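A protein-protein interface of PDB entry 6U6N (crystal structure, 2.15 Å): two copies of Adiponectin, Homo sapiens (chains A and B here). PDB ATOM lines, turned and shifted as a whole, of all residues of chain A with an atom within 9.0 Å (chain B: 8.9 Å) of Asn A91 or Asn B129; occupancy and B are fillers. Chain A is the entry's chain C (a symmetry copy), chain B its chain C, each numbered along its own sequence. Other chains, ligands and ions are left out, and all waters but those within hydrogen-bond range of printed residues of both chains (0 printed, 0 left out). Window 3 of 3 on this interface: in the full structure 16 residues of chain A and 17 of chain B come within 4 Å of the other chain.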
ATOM      1  N   TYR A  61      26.224 -11.648  22.560  1.00  0.00           N
ATOM      2  CA  TYR A  61      27.275 -12.080  23.468  1.00  0.00           C
ATOM      3  C   TYR A  61      28.393 -12.748  22.682  1.00  0.00           C
ATOM      4  O   TYR A  61      28.165 -13.326  21.615  1.00  0.00           O
ATOM      5  CB  TYR A  61      26.736 -13.040  24.534  1.00  0.00           C
ATOM      6  CG  TYR A  61      26.357 -14.406  24.007  1.00  0.00           C
ATOM      7  CD1 TYR A  61      27.271 -15.452  24.017  1.00  0.00           C
ATOM      8  CD2 TYR A  61      25.085 -14.652  23.507  1.00  0.00           C
ATOM      9  CE1 TYR A  61      26.935 -16.699  23.539  1.00  0.00           C
ATOM     10  CE2 TYR A  61      24.736 -15.900  23.028  1.00  0.00           C
ATOM     11  CZ  TYR A  61      25.667 -16.919  23.048  1.00  0.00           C
ATOM     12  OH  TYR A  61      25.339 -18.166  22.576  1.00  0.00           O
ATOM     13  N   LYS A  68      36.041 -28.123  28.656  1.00  0.00           N
ATOM     14  CA  LYS A  68      35.654 -29.192  27.750  1.00  0.00           C
ATOM     15  C   LYS A  68      34.146 -29.396  27.804  1.00  0.00           C
ATOM     16  O   LYS A  68      33.516 -29.217  28.850  1.00  0.00           O
ATOM     17  CB  LYS A  68      36.372 -30.497  28.103  1.00  0.00           C
ATOM     18  N   ASP A  69      33.573 -29.774  26.662  1.00  0.00           N
ATOM     19  CA  ASP A  69      32.132 -29.969  26.515  1.00  0.00           C
ATOM     20  C   ASP A  69      31.370 -28.713  26.940  1.00  0.00           C
ATOM     21  O   ASP A  69      30.495 -28.740  27.808  1.00  0.00           O
ATOM     22  CB  ASP A  69      31.662 -31.197  27.300  1.00  0.00           C
ATOM     23  CG  ASP A  69      32.268 -32.484  26.782  1.00  0.00           C
ATOM     24  OD1 ASP A  69      32.376 -32.637  25.548  1.00  0.00           O
ATOM     25  OD2 ASP A  69      32.640 -33.342  27.610  1.00  0.00           O
ATOM     26  N   VAL A  70      31.730 -27.598  26.304  1.00  0.00           N
ATOM     27  CA  VAL A  70      31.135 -26.312  26.642  1.00  0.00           C
ATOM     28  C   VAL A  70      29.650 -26.315  26.291  1.00  0.00           C
ATOM     29  O   VAL A  70      29.217 -26.931  25.307  1.00  0.00           O
ATOM     30  CB  VAL A  70      31.878 -25.174  25.921  1.00  0.00           C
ATOM     31  CG1 VAL A  70      31.422 -23.819  26.439  1.00  0.00           C
ATOM     32  CG2 VAL A  70      33.382 -25.341  26.085  1.00  0.00           C
ATOM     33  N   LYS A  71      28.859 -25.622  27.109  1.00  0.00           N
ATOM     34  CA  LYS A  71      27.412 -25.533  26.918  1.00  0.00           C
ATOM     35  C   LYS A  71      26.991 -24.119  27.309  1.00  0.00           C
ATOM     36  O   LYS A  71      26.833 -23.819  28.495  1.00  0.00           O
ATOM     37  CB  LYS A  71      26.686 -26.587  27.747  1.00  0.00           C
ATOM     38  CG  LYS A  71      25.365 -27.059  27.164  1.00  0.00           C
ATOM     39  CD  LYS A  71      24.776 -28.185  28.003  1.00  0.00           C
ATOM     40  CE  LYS A  71      23.540 -28.788  27.354  1.00  0.00           C
ATOM     41  NZ  LYS A  71      23.864 -29.549  26.114  1.00  0.00           N
ATOM     42  N   VAL A  72      26.818 -23.255  26.313  1.00  0.00           N
ATOM     43  CA  VAL A  72      26.453 -21.859  26.529  1.00  0.00           C
ATOM     44  C   VAL A  72      24.946 -21.721  26.388  1.00  0.00           C
ATOM     45  O   VAL A  72      24.364 -22.176  25.395  1.00  0.00           O
ATOM     46  CB  VAL A  72      27.182 -20.932  25.541  1.00  0.00           C
ATOM     47  CG1 VAL A  72      26.790 -19.483  25.784  1.00  0.00           C
ATOM     48  CG2 VAL A  72      28.686 -21.109  25.661  1.00  0.00           C
ATOM     49  N   SER A  73      24.310 -21.090  27.373  1.00  0.00           N
ATOM     50  CA  SER A  73      22.864 -20.929  27.385  1.00  0.00           C
ATOM     51  C   SER A  73      22.493 -19.508  27.781  1.00  0.00           C
ATOM     52  O   SER A  73      23.099 -18.926  28.685  1.00  0.00           O
ATOM     53  CB  SER A  73      22.197 -21.919  28.348  1.00  0.00           C
ATOM     54  OG  SER A  73      22.444 -23.257  27.958  1.00  0.00           O
ATOM     55  N   TYR A  88      18.076 -19.751  24.501  1.00  0.00           N
ATOM     56  CA  TYR A  88      19.086 -19.999  23.484  1.00  0.00           C
ATOM     57  C   TYR A  88      20.160 -20.900  24.076  1.00  0.00           C
ATOM     58  O   TYR A  88      20.463 -20.822  25.268  1.00  0.00           O
ATOM     59  CB  TYR A  88      19.700 -18.687  22.977  1.00  0.00           C
ATOM     60  CG  TYR A  88      20.720 -18.870  21.877  1.00  0.00           C
ATOM     61  CD1 TYR A  88      20.344 -18.821  20.545  1.00  0.00           C
ATOM     62  CD2 TYR A  88      22.058 -19.090  22.172  1.00  0.00           C
ATOM     63  CE1 TYR A  88      21.273 -18.987  19.539  1.00  0.00           C
ATOM     64  CE2 TYR A  88      22.988 -19.262  21.171  1.00  0.00           C
ATOM     65  CZ  TYR A  88      22.593 -19.208  19.855  1.00  0.00           C
ATOM     66  OH  TYR A  88      23.522 -19.376  18.853  1.00  0.00           O
ATOM     67  N   GLN A  89      20.738 -21.756  23.232  1.00  0.00           N
ATOM     68  CA  GLN A  89      21.748 -22.698  23.694  1.00  0.00           C
ATOM     69  C   GLN A  89      22.770 -22.965  22.595  1.00  0.00           C
ATOM     70  O   GLN A  89      22.412 -23.088  21.420  1.00  0.00           O
ATOM     71  CB  GLN A  89      21.110 -24.017  24.146  1.00  0.00           C
ATOM     72  N   GLU A  90      24.039 -23.055  22.991  1.00  0.00           N
ATOM     73  CA  GLU A  90      25.127 -23.470  22.116  1.00  0.00           C
ATOM     74  C   GLU A  90      25.929 -24.564  22.808  1.00  0.00           C
ATOM     75  O   GLU A  90      26.052 -24.579  24.035  1.00  0.00           O
ATOM     76  CB  GLU A  90      26.047 -22.297  21.748  1.00  0.00           C
ATOM     77  CG  GLU A  90      25.589 -21.508  20.531  1.00  0.00           C
ATOM     78  CD  GLU A  90      26.522 -20.362  20.189  1.00  0.00           C
ATOM     79  OE1 GLU A  90      26.900 -19.602  21.106  1.00  0.00           O
ATOM     80  OE2 GLU A  90      26.883 -20.224  19.001  1.00  0.00           O
ATOM     81  N   ASN A  91      26.478 -25.481  22.012  1.00  0.00           N
ATOM     82  CA  ASN A  91      27.142 -26.664  22.544  1.00  0.00           C
ATOM     83  C   ASN A  91      28.482 -26.895  21.862  1.00  0.00           C
ATOM     84  O   ASN A  91      28.619 -26.695  20.652  1.00  0.00           O
ATOM     85  CB  ASN A  91      26.260 -27.908  22.376  1.00  0.00           C
ATOM     86  CG  ASN A  91      25.134 -27.963  23.387  1.00  0.00           C
ATOM     87  OD1 ASN A  91      25.230 -28.658  24.397  1.00  0.00           O
ATOM     88  ND2 ASN A  91      24.061 -27.227  23.123  1.00  0.00           N
ATOM     89  N   ASN A  92      29.466 -27.326  22.655  1.00  0.00           N
ATOM     90  CA  ASN A  92      30.766 -27.777  22.157  1.00  0.00           C
ATOM     91  C   ASN A  92      31.432 -26.721  21.275  1.00  0.00           C
ATOM     92  O   ASN A  92      31.889 -26.998  20.164  1.00  0.00           O
ATOM     93  CB  ASN A  92      30.628 -29.105  21.410  1.00  0.00           C
ATOM     94  N   VAL A  93      31.482 -25.492  21.783  1.00  0.00           N
ATOM     95  CA  VAL A  93      32.118 -24.377  21.091  1.00  0.00           C
ATOM     96  C   VAL A  93      33.019 -23.658  22.083  1.00  0.00           C
ATOM     97  O   VAL A  93      32.549 -23.190  23.128  1.00  0.00           O
ATOM     98  CB  VAL A  93      31.091 -23.401  20.491  1.00  0.00           C
ATOM     99  CG1 VAL A  93      31.800 -22.252  19.803  1.00  0.00           C
ATOM    100  CG2 VAL A  93      30.174 -24.119  19.512  1.00  0.00           C
ATOM    101  N   ASP A  94      34.312 -23.569  21.762  1.00  0.00           N
ATOM    102  CA  ASP A  94      35.247 -22.884  22.649  1.00  0.00           C
ATOM    103  C   ASP A  94      35.019 -21.378  22.636  1.00  0.00           C
ATOM    104  O   ASP A  94      35.007 -20.737  23.693  1.00  0.00           O
ATOM    105  CB  ASP A  94      36.686 -23.215  22.250  1.00  0.00           C
ATOM    106  CG  ASP A  94      37.038 -24.670  22.493  1.00  0.00           C
ATOM    107  OD1 ASP A  94      36.583 -25.230  23.514  1.00  0.00           O
ATOM    108  OD2 ASP A  94      37.768 -25.252  21.664  1.00  0.00           O
ATOM    109  N   GLN A  95      34.839 -20.796  21.455  1.00  0.00           N
ATOM    110  CA  GLN A  95      34.577 -19.367  21.297  1.00  0.00           C
ATOM    111  C   GLN A  95      33.149 -19.220  20.777  1.00  0.00           C
ATOM    112  O   GLN A  95      32.910 -19.201  19.569  1.00  0.00           O
ATOM    113  CB  GLN A  95      35.591 -18.721  20.357  1.00  0.00           C
ATOM    114  N   ALA A  96      32.198 -19.113  21.701  1.00  0.00           N
ATOM    115  CA  ALA A  96      30.785 -19.060  21.357  1.00  0.00           C
ATOM    116  C   ALA A  96      30.335 -17.618  21.173  1.00  0.00           C
ATOM    117  O   ALA A  96      30.573 -16.769  22.039  1.00  0.00           O
ATOM    118  CB  ALA A  96      29.945 -19.742  22.437  1.00  0.00           C
ATOM    119  N   SER A  97      29.686 -17.348  20.044  1.00  0.00           N
ATOM    120  CA  SER A  97      29.081 -16.056  19.759  1.00  0.00           C
ATOM    121  C   SER A  97      27.613 -16.256  19.411  1.00  0.00           C
ATOM    122  O   SER A  97      27.221 -17.304  18.888  1.00  0.00           O
ATOM    123  CB  SER A  97      29.800 -15.339  18.607  1.00  0.00           C
ATOM    124  OG  SER A  97      31.166 -15.123  18.909  1.00  0.00           O
ATOM    125  N   VAL A 114      27.034 -20.945  31.463  1.00  0.00           N
ATOM    126  CA  VAL A 114      27.921 -21.867  30.765  1.00  0.00           C
ATOM    127  C   VAL A 114      28.068 -23.129  31.604  1.00  0.00           C
ATOM    128  O   VAL A 114      28.047 -23.073  32.838  1.00  0.00           O
ATOM    129  CB  VAL A 114      29.297 -21.224  30.480  1.00  0.00           C
ATOM    130  CG1 VAL A 114      30.043 -20.919  31.780  1.00  0.00           C
ATOM    131  CG2 VAL A 114      30.130 -22.110  29.565  1.00  0.00           C
ATOM    132  N   TYR A 115      28.184 -24.272  30.932  1.00  0.00           N
ATOM    133  CA  TYR A 115      28.488 -25.541  31.576  1.00  0.00           C
ATOM    134  C   TYR A 115      29.705 -26.163  30.908  1.00  0.00           C
ATOM    135  O   TYR A 115      29.889 -26.038  29.693  1.00  0.00           O
ATOM    136  CB  TYR A 115      27.306 -26.516  31.506  1.00  0.00           C
ATOM    137  CG  TYR A 115      27.677 -27.932  31.896  1.00  0.00           C
ATOM    138  CD1 TYR A 115      27.848 -28.283  33.229  1.00  0.00           C
ATOM    139  CD2 TYR A 115      27.867 -28.914  30.931  1.00  0.00           C
ATOM    140  CE1 TYR A 115      28.193 -29.573  33.591  1.00  0.00           C
ATOM    141  CE2 TYR A 115      28.212 -30.208  31.285  1.00  0.00           C
ATOM    142  CZ  TYR A 115      28.372 -30.531  32.616  1.00  0.00           C
ATOM    143  OH  TYR A 115      28.715 -31.816  32.972  1.00  0.00           O
ATOM    144  N   GLY B  17      16.074 -19.307  14.330  1.00  0.00           N
ATOM    145  CA  GLY B  17      17.111 -20.289  14.571  1.00  0.00           C
ATOM    146  C   GLY B  17      16.882 -21.564  13.776  1.00  0.00           C
ATOM    147  O   GLY B  17      15.908 -21.691  13.030  1.00  0.00           O
ATOM    148  N   LEU B  18      17.801 -22.510  13.964  1.00  0.00           N
ATOM    149  CA  LEU B  18      17.781 -23.754  13.199  1.00  0.00           C
ATOM    150  C   LEU B  18      17.944 -24.995  14.066  1.00  0.00           C
ATOM    151  O   LEU B  18      17.272 -26.001  13.815  1.00  0.00           O
ATOM    152  CB  LEU B  18      18.880 -23.713  12.125  1.00  0.00           C
ATOM    153  CG  LEU B  18      18.864 -24.829  11.078  1.00  0.00           C
ATOM    154  CD1 LEU B  18      17.535 -24.863  10.340  1.00  0.00           C
ATOM    155  CD2 LEU B  18      20.016 -24.662  10.102  1.00  0.00           C
ATOM    156  N   GLU B  19      18.830 -24.955  15.064  1.00  0.00           N
ATOM    157  CA  GLU B  19      19.066 -26.036  16.022  1.00  0.00           C
ATOM    158  C   GLU B  19      19.691 -27.280  15.397  1.00  0.00           C
ATOM    159  O   GLU B  19      19.594 -28.370  15.970  1.00  0.00           O
ATOM    160  CB  GLU B  19      17.782 -26.443  16.759  1.00  0.00           C
ATOM    161  CG  GLU B  19      17.080 -25.326  17.501  1.00  0.00           C
ATOM    162  CD  GLU B  19      16.038 -25.853  18.471  1.00  0.00           C
ATOM    163  OE1 GLU B  19      16.410 -26.612  19.391  1.00  0.00           O
ATOM    164  OE2 GLU B  19      14.845 -25.522  18.305  1.00  0.00           O
ATOM    165  N   THR B  20      20.336 -27.163  14.236  1.00  0.00           N
ATOM    166  CA  THR B  20      21.006 -28.296  13.609  1.00  0.00           C
ATOM    167  C   THR B  20      22.446 -27.914  13.282  1.00  0.00           C
ATOM    168  O   THR B  20      22.871 -26.769  13.466  1.00  0.00           O
ATOM    169  CB  THR B  20      20.268 -28.769  12.348  1.00  0.00           C
ATOM    170  OG1 THR B  20      20.172 -27.690  11.411  1.00  0.00           O
ATOM    171  CG2 THR B  20      18.870 -29.267  12.693  1.00  0.00           C
ATOM    172  N   TYR B  21      23.202 -28.897  12.788  1.00  0.00           N
ATOM    173  CA  TYR B  21      24.624 -28.702  12.528  1.00  0.00           C
ATOM    174  C   TYR B  21      24.863 -28.014  11.190  1.00  0.00           C
ATOM    175  O   TYR B  21      25.516 -26.967  11.134  1.00  0.00           O
ATOM    176  CB  TYR B  21      25.356 -30.043  12.577  1.00  0.00           C
ATOM    177  N   VAL B  22      24.348 -28.584  10.101  1.00  0.00           N
ATOM    178  CA  VAL B  22      24.550 -28.017   8.772  1.00  0.00           C
ATOM    179  C   VAL B  22      23.331 -28.299   7.907  1.00  0.00           C
ATOM    180  O   VAL B  22      23.009 -29.459   7.627  1.00  0.00           O
ATOM    181  CB  VAL B  22      25.827 -28.570   8.114  1.00  0.00           C
ATOM    182  N   LYS B  33      13.102 -22.523  13.810  1.00  0.00           N
ATOM    183  CA  LYS B  33      12.879 -21.966  15.138  1.00  0.00           C
ATOM    184  C   LYS B  33      12.675 -20.459  15.039  1.00  0.00           C
ATOM    185  O   LYS B  33      13.423 -19.766  14.344  1.00  0.00           O
ATOM    186  CB  LYS B  33      14.059 -22.284  16.054  1.00  0.00           C
ATOM    187  CG  LYS B  33      13.800 -21.981  17.523  1.00  0.00           C
ATOM    188  CD  LYS B  33      14.983 -22.382  18.389  1.00  0.00           C
ATOM    189  CE  LYS B  33      14.606 -22.391  19.864  1.00  0.00           C
ATOM    190  NZ  LYS B  33      15.716 -22.889  20.726  1.00  0.00           N
ATOM    191  N   PHE B  35      12.348 -17.041  17.210  1.00  0.00           N
ATOM    192  CA  PHE B  35      12.451 -16.318  18.473  1.00  0.00           C
ATOM    193  C   PHE B  35      11.535 -15.102  18.491  1.00  0.00           C
ATOM    194  O   PHE B  35      10.921 -14.796  19.520  1.00  0.00           O
ATOM    195  CB  PHE B  35      13.898 -15.892  18.731  1.00  0.00           C
ATOM    196  CG  PHE B  35      14.871 -17.037  18.785  1.00  0.00           C
ATOM    197  CD1 PHE B  35      15.706 -17.301  17.712  1.00  0.00           C
ATOM    198  CD2 PHE B  35      14.957 -17.844  19.910  1.00  0.00           C
ATOM    199  CE1 PHE B  35      16.604 -18.349  17.755  1.00  0.00           C
ATOM    200  CE2 PHE B  35      15.855 -18.895  19.959  1.00  0.00           C
ATOM    201  CZ  PHE B  35      16.679 -19.148  18.880  1.00  0.00           C
ATOM    202  N   HIS B  62      24.920 -16.010  13.216  1.00  0.00           N
ATOM    203  CA  HIS B  62      25.949 -16.868  13.805  1.00  0.00           C
ATOM    204  C   HIS B  62      25.619 -18.298  13.389  1.00  0.00           C
ATOM    205  O   HIS B  62      24.789 -18.955  14.024  1.00  0.00           O
ATOM    206  CB  HIS B  62      25.995 -16.726  15.322  1.00  0.00           C
ATOM    207  CG  HIS B  62      26.131 -15.312  15.795  1.00  0.00           C
ATOM    208  ND1 HIS B  62      25.095 -14.404  15.739  1.00  0.00           N
ATOM    209  CD2 HIS B  62      27.181 -14.651  16.338  1.00  0.00           C
ATOM    210  CE1 HIS B  62      25.503 -13.243  16.222  1.00  0.00           C
ATOM    211  NE2 HIS B  62      26.764 -13.367  16.593  1.00  0.00           N
ATOM    212  N   ILE B  63      26.266 -18.777  12.330  1.00  0.00           N
ATOM    213  CA  ILE B  63      25.944 -20.060  11.716  1.00  0.00           C
ATOM    214  C   ILE B  63      27.060 -21.051  12.012  1.00  0.00           C
ATOM    215  O   ILE B  63      28.244 -20.737  11.834  1.00  0.00           O
ATOM    216  CB  ILE B  63      25.733 -19.921  10.198  1.00  0.00           C
ATOM    217  CG1 ILE B  63      24.689 -18.843   9.897  1.00  0.00           C
ATOM    218  CG2 ILE B  63      25.320 -21.254   9.592  1.00  0.00           C
ATOM    219  CD1 ILE B  63      23.363 -19.063  10.585  1.00  0.00           C
ATOM    220  N   THR B  64      26.682 -22.243  12.465  1.00  0.00           N
ATOM    221  CA  THR B  64      27.586 -23.380  12.565  1.00  0.00           C
ATOM    222  C   THR B  64      27.396 -24.258  11.338  1.00  0.00           C
ATOM    223  O   THR B  64      26.273 -24.416  10.847  1.00  0.00           O
ATOM    224  CB  THR B  64      27.319 -24.184  13.842  1.00  0.00           C
ATOM    225  OG1 THR B  64      27.413 -23.318  14.979  1.00  0.00           O
ATOM    226  CG2 THR B  64      28.326 -25.315  13.991  1.00  0.00           C
ATOM    227  N   VAL B  65      28.493 -24.809  10.821  1.00  0.00           N
ATOM    228  CA  VAL B  65      28.458 -25.600   9.595  1.00  0.00           C
ATOM    229  C   VAL B  65      29.300 -26.854   9.781  1.00  0.00           C
ATOM    230  O   VAL B  65      30.448 -26.779  10.233  1.00  0.00           O
ATOM    231  CB  VAL B  65      28.957 -24.801   8.375  1.00  0.00           C
ATOM    232  CG1 VAL B  65      28.914 -25.668   7.131  1.00  0.00           C
ATOM    233  CG2 VAL B  65      28.123 -23.543   8.172  1.00  0.00           C
ATOM    234  N   TYR B  66      28.727 -28.005   9.429  1.00  0.00           N
ATOM    235  CA  TYR B  66      29.435 -29.278   9.417  1.00  0.00           C
ATOM    236  C   TYR B  66      29.703 -29.685   7.971  1.00  0.00           C
ATOM    237  O   TYR B  66      29.196 -30.704   7.491  1.00  0.00           O
ATOM    238  CB  TYR B  66      28.621 -30.338  10.173  1.00  0.00           C
ATOM    239  CG  TYR B  66      29.155 -31.756  10.104  1.00  0.00           C
ATOM    240  CD1 TYR B  66      30.431 -32.068  10.552  1.00  0.00           C
ATOM    241  CD2 TYR B  66      28.368 -32.786   9.602  1.00  0.00           C
ATOM    242  CE1 TYR B  66      30.912 -33.367  10.491  1.00  0.00           C
ATOM    243  CE2 TYR B  66      28.839 -34.083   9.537  1.00  0.00           C
ATOM    244  CZ  TYR B  66      30.110 -34.368   9.983  1.00  0.00           C
ATOM    245  OH  TYR B  66      30.579 -35.660   9.918  1.00  0.00           O
ATOM    246  N   ASP B  94      34.215 -22.701   9.748  1.00  0.00           N
ATOM    247  CA  ASP B  94      33.261 -23.659  10.298  1.00  0.00           C
ATOM    248  C   ASP B  94      32.193 -22.961  11.132  1.00  0.00           C
ATOM    249  O   ASP B  94      31.003 -23.268  11.011  1.00  0.00           O
ATOM    250  CB  ASP B  94      33.994 -24.711  11.130  1.00  0.00           C
ATOM    251  CG  ASP B  94      34.881 -25.607  10.288  1.00  0.00           C
ATOM    252  OD1 ASP B  94      34.476 -25.953   9.157  1.00  0.00           O
ATOM    253  OD2 ASP B  94      35.982 -25.964  10.755  1.00  0.00           O
ATOM    254  N   GLN B  95      32.599 -22.023  11.982  1.00  0.00           N
ATOM    255  CA  GLN B  95      31.684 -21.250  12.818  1.00  0.00           C
ATOM    256  C   GLN B  95      31.728 -19.805  12.329  1.00  0.00           C
ATOM    257  O   GLN B  95      32.532 -18.998  12.798  1.00  0.00           O
ATOM    258  CB  GLN B  95      32.060 -21.360  14.294  1.00  0.00           C
ATOM    259  N   ASN B 129      23.470 -27.249  18.622  1.00  0.00           N
ATOM    260  CA  ASN B 129      24.039 -26.025  18.068  1.00  0.00           C
ATOM    261  C   ASN B 129      22.967 -25.144  17.438  1.00  0.00           C
ATOM    262  O   ASN B 129      22.352 -25.519  16.440  1.00  0.00           O
ATOM    263  CB  ASN B 129      25.114 -26.353  17.032  1.00  0.00           C
ATOM    264  CG  ASN B 129      26.359 -26.944  17.656  1.00  0.00           C
ATOM    265  OD1 ASN B 129      26.635 -26.723  18.833  1.00  0.00           O
ATOM    266  ND2 ASN B 129      27.120 -27.695  16.869  1.00  0.00           N
ATOM    267  N   ASP B 130      22.750 -23.970  18.026  1.00  0.00           N
ATOM    268  CA  ASP B 130      21.771 -23.019  17.519  1.00  0.00           C
ATOM    269  C   ASP B 130      22.455 -22.034  16.579  1.00  0.00           C
ATOM    270  O   ASP B 130      23.364 -21.304  16.989  1.00  0.00           O
ATOM    271  CB  ASP B 130      21.087 -22.273  18.663  1.00  0.00           C
ATOM    272  CG  ASP B 130      19.992 -23.087  19.321  1.00  0.00           C
ATOM    273  OD1 ASP B 130      19.783 -24.247  18.910  1.00  0.00           O
ATOM    274  OD2 ASP B 130      19.338 -22.564  20.247  1.00  0.00           O
ATOM    275  N   SER B 131      22.018 -22.018  15.324  1.00  0.00           N
ATOM    276  CA  SER B 131      22.461 -21.037  14.347  1.00  0.00           C
ATOM    277  C   SER B 131      21.363 -19.998  14.169  1.00  0.00           C
ATOM    278  O   SER B 131      20.220 -20.348  13.861  1.00  0.00           O
ATOM    279  CB  SER B 131      22.787 -21.703  13.010  1.00  0.00           C
ATOM    280  OG  SER B 131      23.778 -22.705  13.169  1.00  0.00           O
ATOM    281  N   THR B 132      21.707 -18.729  14.363  1.00  0.00           N
ATOM    282  CA  THR B 132      20.718 -17.663  14.382  1.00  0.00           C
ATOM    283  C   THR B 132      20.852 -16.746  13.175  1.00  0.00           C
ATOM    284  O   THR B 132      21.867 -16.727  12.475  1.00  0.00           O
ATOM    285  CB  THR B 132      20.828 -16.831  15.662  1.00  0.00           C
ATOM    286  OG1 THR B 132      22.206 -16.691  16.033  1.00  0.00           O
ATOM    287  CG2 THR B 132      20.053 -17.490  16.785  1.00  0.00           C
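Tyr A88 touches Thr B132 (CE1 to CG2, 3.4 Å).
Ser A97 touches His B62 (C to CD2, 3.5 Å).
The backbone carbonyl oxygen of Asp B130 is in hydrogen-bond range of the side-chain hydroxyl of Tyr A88 (2.7 Å).
The side-chain carboxylate (OD2) of Asp B130 sits at hydrogen-bond distance from the backbone NH (N) of Gln A89.
O of Asn A91 lies close to OD1 of Asn B129 (2.7 Å).
Positions printed for both chains: 94 and 95.
Of the 5 pairs that touch across the chains among the printed residues, none has its exchanged pair printed and touching as well.
The backbone NH (N) of Thr B20 sits at hydrogen-bond distance from the backbone carbonyl oxygen (O) of Asn B129 (3.4 Å).
The backbone NH of Thr B132 lies within hydrogen-bond range of the backbone carbonyl oxygen of His B62 (3.1 Å).
The side-chain amino group (NZ) of Lys B33 is in salt-bridge range of the side-chain carboxylate (OD2) of Asp B130, 3.7 Å away.
The side-chain carboxylate (OE2) of Glu A90 sits close to the side-chain hydroxyl (OH) of Tyr A88 (3.5 Å).
Printed residues of chain A that touch a printed residue of chain B: Tyr A88, Gln A89, Asn A91 and Ser A97.
Hydrophobic or aromatic side chains of chain A that line the printed part of chain B: Tyr A88.
Hydrophobic or aromatic side chains of chain B within 4 Å of the printed part of chain A: His B62.
Among the printed residues, 5 pairs touch across the chains.
Printed residues of chain B within 4 Å of Tyr A88: Asp B130 (2.7 Å) and Thr B132 (3.4 Å).
Asn A91 touches just one residue of chain B: Asn B129.
Lys B33 touches none of the printed residues of chain A.
Printed residues of chain A within 4 Å of His B62: Ser A97.
Of chain A, only Asn A91 (2.7 Å) comes within 4 Å of Asn B129.
Printed residues of chain A within 4 Å of Thr B132: Tyr A88 (3.4 Å).
The nearest residue of chain A that does not touch Asn B129 is Val A93 (4.4 Å).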
